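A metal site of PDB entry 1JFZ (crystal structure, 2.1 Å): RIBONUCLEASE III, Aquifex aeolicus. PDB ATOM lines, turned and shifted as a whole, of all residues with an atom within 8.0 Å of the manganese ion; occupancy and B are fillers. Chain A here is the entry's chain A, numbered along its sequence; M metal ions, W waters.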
ATOM      1  N   TYR A  37     -11.288  12.409 -22.452  1.00  0.00           N
ATOM      2  CA  TYR A  37     -11.843  13.748 -22.492  1.00  0.00           C
ATOM      3  C   TYR A  37     -13.113  13.914 -23.320  1.00  0.00           C
ATOM      4  O   TYR A  37     -13.707  14.995 -23.238  1.00  0.00           O
ATOM      5  CB  TYR A  37     -10.777  14.740 -22.996  1.00  0.00           C
ATOM      6  CG  TYR A  37     -10.226  14.586 -24.384  1.00  0.00           C
ATOM      7  CD1 TYR A  37     -10.913  15.024 -25.508  1.00  0.00           C
ATOM      8  CD2 TYR A  37      -8.979  14.029 -24.621  1.00  0.00           C
ATOM      9  CE1 TYR A  37     -10.431  14.899 -26.791  1.00  0.00           C
ATOM     10  CE2 TYR A  37      -8.468  13.895 -25.898  1.00  0.00           C
ATOM     11  CZ  TYR A  37      -9.182  14.324 -26.992  1.00  0.00           C
ATOM     12  OH  TYR A  37      -8.706  14.206 -28.270  1.00  0.00           O
ATOM     13  N   GLU A  38     -13.503  12.935 -24.108  1.00  0.00           N
ATOM     14  CA  GLU A  38     -14.607  13.062 -25.062  1.00  0.00           C
ATOM     15  C   GLU A  38     -15.857  13.725 -24.508  1.00  0.00           C
ATOM     16  O   GLU A  38     -16.500  14.522 -25.183  1.00  0.00           O
ATOM     17  CB  GLU A  38     -15.006  11.691 -25.605  1.00  0.00           C
ATOM     18  CG  GLU A  38     -15.879  11.722 -26.850  1.00  0.00           C
ATOM     19  CD  GLU A  38     -16.458  10.335 -27.125  1.00  0.00           C
ATOM     20  OE1 GLU A  38     -15.656   9.406 -27.354  1.00  0.00           O
ATOM     21  OE2 GLU A  38     -17.688  10.179 -27.088  1.00  0.00           O
ATOM     22  N   GLU A  41     -14.963  17.476 -23.629  1.00  0.00           N
ATOM     23  CA  GLU A  41     -14.821  18.206 -24.884  1.00  0.00           C
ATOM     24  C   GLU A  41     -16.211  18.633 -25.369  1.00  0.00           C
ATOM     25  O   GLU A  41     -16.397  19.775 -25.799  1.00  0.00           O
ATOM     26  CB  GLU A  41     -14.170  17.348 -25.972  1.00  0.00           C
ATOM     27  CG  GLU A  41     -14.033  18.059 -27.302  1.00  0.00           C
ATOM     28  CD  GLU A  41     -13.882  17.114 -28.487  1.00  0.00           C
ATOM     29  OE1 GLU A  41     -13.749  15.892 -28.270  1.00  0.00           O
ATOM     30  OE2 GLU A  41     -13.908  17.607 -29.637  1.00  0.00           O
ATOM     31  N   PHE A  42     -17.159  17.703 -25.286  1.00  0.00           N
ATOM     32  CA  PHE A  42     -18.513  18.024 -25.747  1.00  0.00           C
ATOM     33  C   PHE A  42     -19.034  19.270 -25.033  1.00  0.00           C
ATOM     34  O   PHE A  42     -19.597  20.163 -25.644  1.00  0.00           O
ATOM     35  CB  PHE A  42     -19.467  16.862 -25.541  1.00  0.00           C
ATOM     36  CG  PHE A  42     -20.775  16.935 -26.323  1.00  0.00           C
ATOM     37  CD1 PHE A  42     -20.786  16.963 -27.709  1.00  0.00           C
ATOM     38  CD2 PHE A  42     -21.988  16.956 -25.657  1.00  0.00           C
ATOM     39  CE1 PHE A  42     -21.979  17.012 -28.408  1.00  0.00           C
ATOM     40  CE2 PHE A  42     -23.187  17.008 -26.344  1.00  0.00           C
ATOM     41  CZ  PHE A  42     -23.184  17.034 -27.731  1.00  0.00           C
ATOM     42  N   GLY A  44     -17.185  21.554 -23.195  1.00  0.00           N
ATOM     43  CA  GLY A  44     -16.277  22.686 -23.335  1.00  0.00           C
ATOM     44  C   GLY A  44     -16.448  23.371 -24.675  1.00  0.00           C
ATOM     45  O   GLY A  44     -16.203  24.560 -24.824  1.00  0.00           O
ATOM     46  N   ASP A  45     -16.883  22.577 -25.648  1.00  0.00           N
ATOM     47  CA  ASP A  45     -17.182  23.079 -26.982  1.00  0.00           C
ATOM     48  C   ASP A  45     -18.242  24.170 -26.896  1.00  0.00           C
ATOM     49  O   ASP A  45     -18.102  25.266 -27.441  1.00  0.00           O
ATOM     50  CB  ASP A  45     -17.661  21.904 -27.837  1.00  0.00           C
ATOM     51  CG  ASP A  45     -17.906  22.236 -29.288  1.00  0.00           C
ATOM     52  OD1 ASP A  45     -18.216  23.406 -29.588  1.00  0.00           O
ATOM     53  OD2 ASP A  45     -17.774  21.340 -30.148  1.00  0.00           O
ATOM     54  N   PHE A  81      -7.709  27.957 -31.820  1.00  0.00           N
ATOM     55  CA  PHE A  81      -7.684  27.318 -30.496  1.00  0.00           C
ATOM     56  C   PHE A  81      -6.287  26.803 -30.198  1.00  0.00           C
ATOM     57  O   PHE A  81      -5.878  26.680 -29.042  1.00  0.00           O
ATOM     58  CB  PHE A  81      -8.679  26.169 -30.349  1.00  0.00           C
ATOM     59  CG  PHE A  81     -10.111  26.551 -30.044  1.00  0.00           C
ATOM     60  CD1 PHE A  81     -10.563  27.845 -30.188  1.00  0.00           C
ATOM     61  CD2 PHE A  81     -11.016  25.583 -29.613  1.00  0.00           C
ATOM     62  CE1 PHE A  81     -11.867  28.187 -29.908  1.00  0.00           C
ATOM     63  CE2 PHE A  81     -12.331  25.907 -29.341  1.00  0.00           C
ATOM     64  CZ  PHE A  81     -12.761  27.213 -29.503  1.00  0.00           C
ATOM     65  N   THR A 104      -5.685  19.040 -33.923  1.00  0.00           N
ATOM     66  CA  THR A 104      -7.077  18.693 -33.727  1.00  0.00           C
ATOM     67  C   THR A 104      -7.337  18.230 -32.293  1.00  0.00           C
ATOM     68  O   THR A 104      -8.264  18.729 -31.655  1.00  0.00           O
ATOM     69  CB  THR A 104      -7.550  17.588 -34.682  1.00  0.00           C
ATOM     70  OG1 THR A 104      -7.362  18.002 -36.047  1.00  0.00           O
ATOM     71  CG2 THR A 104      -9.040  17.326 -34.506  1.00  0.00           C
ATOM     72  N   ILE A 105      -6.512  17.296 -31.848  1.00  0.00           N
ATOM     73  CA  ILE A 105      -6.506  16.753 -30.499  1.00  0.00           C
ATOM     74  C   ILE A 105      -6.193  17.829 -29.462  1.00  0.00           C
ATOM     75  O   ILE A 105      -6.850  17.945 -28.420  1.00  0.00           O
ATOM     76  CB  ILE A 105      -5.518  15.572 -30.414  1.00  0.00           C
ATOM     77  CG1 ILE A 105      -5.964  14.356 -31.246  1.00  0.00           C
ATOM     78  CG2 ILE A 105      -5.259  15.148 -28.975  1.00  0.00           C
ATOM     79  CD1 ILE A 105      -4.937  13.233 -31.268  1.00  0.00           C
ATOM     80  N   GLY A 107      -6.795  20.834 -29.874  1.00  0.00           N
ATOM     81  CA  GLY A 107      -8.003  21.623 -30.027  1.00  0.00           C
ATOM     82  C   GLY A 107      -9.160  21.086 -29.199  1.00  0.00           C
ATOM     83  O   GLY A 107      -9.919  21.883 -28.625  1.00  0.00           O
ATOM     84  N   ASP A 108      -9.282  19.772 -29.127  1.00  0.00           N
ATOM     85  CA  ASP A 108     -10.270  19.059 -28.337  1.00  0.00           C
ATOM     86  C   ASP A 108      -9.913  18.965 -26.865  1.00  0.00           C
ATOM     87  O   ASP A 108     -10.782  18.917 -26.004  1.00  0.00           O
ATOM     88  CB  ASP A 108     -10.462  17.621 -28.866  1.00  0.00           C
ATOM     89  CG  ASP A 108     -11.056  17.618 -30.262  1.00  0.00           C
ATOM     90  OD1 ASP A 108     -11.647  18.648 -30.627  1.00  0.00           O
ATOM     91  OD2 ASP A 108     -10.914  16.603 -30.958  1.00  0.00           O
ATOM     92  N   VAL A 109      -8.629  18.902 -26.532  1.00  0.00           N
ATOM     93  CA  VAL A 109      -8.289  18.869 -25.097  1.00  0.00           C
ATOM     94  C   VAL A 109      -8.574  20.255 -24.516  1.00  0.00           C
ATOM     95  O   VAL A 109      -9.014  20.390 -23.375  1.00  0.00           O
ATOM     96  CB  VAL A 109      -6.833  18.463 -24.871  1.00  0.00           C
ATOM     97  CG1 VAL A 109      -6.336  18.877 -23.494  1.00  0.00           C
ATOM     98  CG2 VAL A 109      -6.665  16.948 -25.009  1.00  0.00           C
ATOM     99  N   PHE A 110      -8.311  21.253 -25.347  1.00  0.00           N
ATOM    100  CA  PHE A 110      -8.507  22.644 -24.934  1.00  0.00           C
ATOM    101  C   PHE A 110      -9.953  22.851 -24.524  1.00  0.00           C
ATOM    102  O   PHE A 110     -10.259  23.328 -23.424  1.00  0.00           O
ATOM    103  CB  PHE A 110      -8.044  23.547 -26.076  1.00  0.00           C
ATOM    104  CG  PHE A 110      -8.139  25.034 -25.777  1.00  0.00           C
ATOM    105  CD1 PHE A 110      -7.201  25.676 -24.977  1.00  0.00           C
ATOM    106  CD2 PHE A 110      -9.175  25.784 -26.312  1.00  0.00           C
ATOM    107  CE1 PHE A 110      -7.308  27.027 -24.721  1.00  0.00           C
ATOM    108  CE2 PHE A 110      -9.282  27.139 -26.065  1.00  0.00           C
ATOM    109  CZ  PHE A 110      -8.333  27.762 -25.263  1.00  0.00           C
ATOM    110  N   GLU A 111     -10.913  22.471 -25.363  1.00  0.00           N
ATOM    111  CA  GLU A 111     -12.319  22.523 -24.962  1.00  0.00           C
ATOM    112  C   GLU A 111     -12.528  21.717 -23.685  1.00  0.00           C
ATOM    113  O   GLU A 111     -13.335  22.069 -22.823  1.00  0.00           O
ATOM    114  CB  GLU A 111     -13.224  22.014 -26.077  1.00  0.00           C
ATOM    115  CG  GLU A 111     -13.048  22.706 -27.418  1.00  0.00           C
ATOM    116  CD  GLU A 111     -13.696  21.988 -28.590  1.00  0.00           C
ATOM    117  OE1 GLU A 111     -13.893  20.758 -28.529  1.00  0.00           O
ATOM    118  OE2 GLU A 111     -14.005  22.676 -29.588  1.00  0.00           O
ATOM    119  N   ALA A 112     -11.799  20.607 -23.565  1.00  0.00           N
ATOM    120  CA  ALA A 112     -12.035  19.727 -22.423  1.00  0.00           C
ATOM    121  C   ALA A 112     -11.569  20.370 -21.112  1.00  0.00           C
ATOM    122  O   ALA A 112     -12.255  20.310 -20.087  1.00  0.00           O
ATOM    123  CB  ALA A 112     -11.322  18.393 -22.632  1.00  0.00           C
HETATM  124 MN    MN M   1     -13.901  19.522 -30.358  1.00  0.00          MN
HETATM  125  O   HOH W   1     -13.683  21.217 -31.684  1.00  0.00           O
HETATM  126  O   HOH W   2     -14.478  18.223 -32.169  1.00  0.00           O
HETATM  127  O   HOH W   3     -16.200  19.679 -30.032  1.00  0.00           O
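OE2 of Glu 41 binds the manganese ion (2.0 Å).
Water W1 binds the manganese ion (2.2 Å).
OE1 of Glu 111 binds the manganese ion.
Water W2 binds the manganese ion, 2.3 Å away.
Water W3 is bound to the manganese ion.
OD1 of Asp 108 binds the manganese ion, at 2.4 Å.
The nearest printed residue that does not touch the manganese ion is Asp 45 (4.3 Å).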
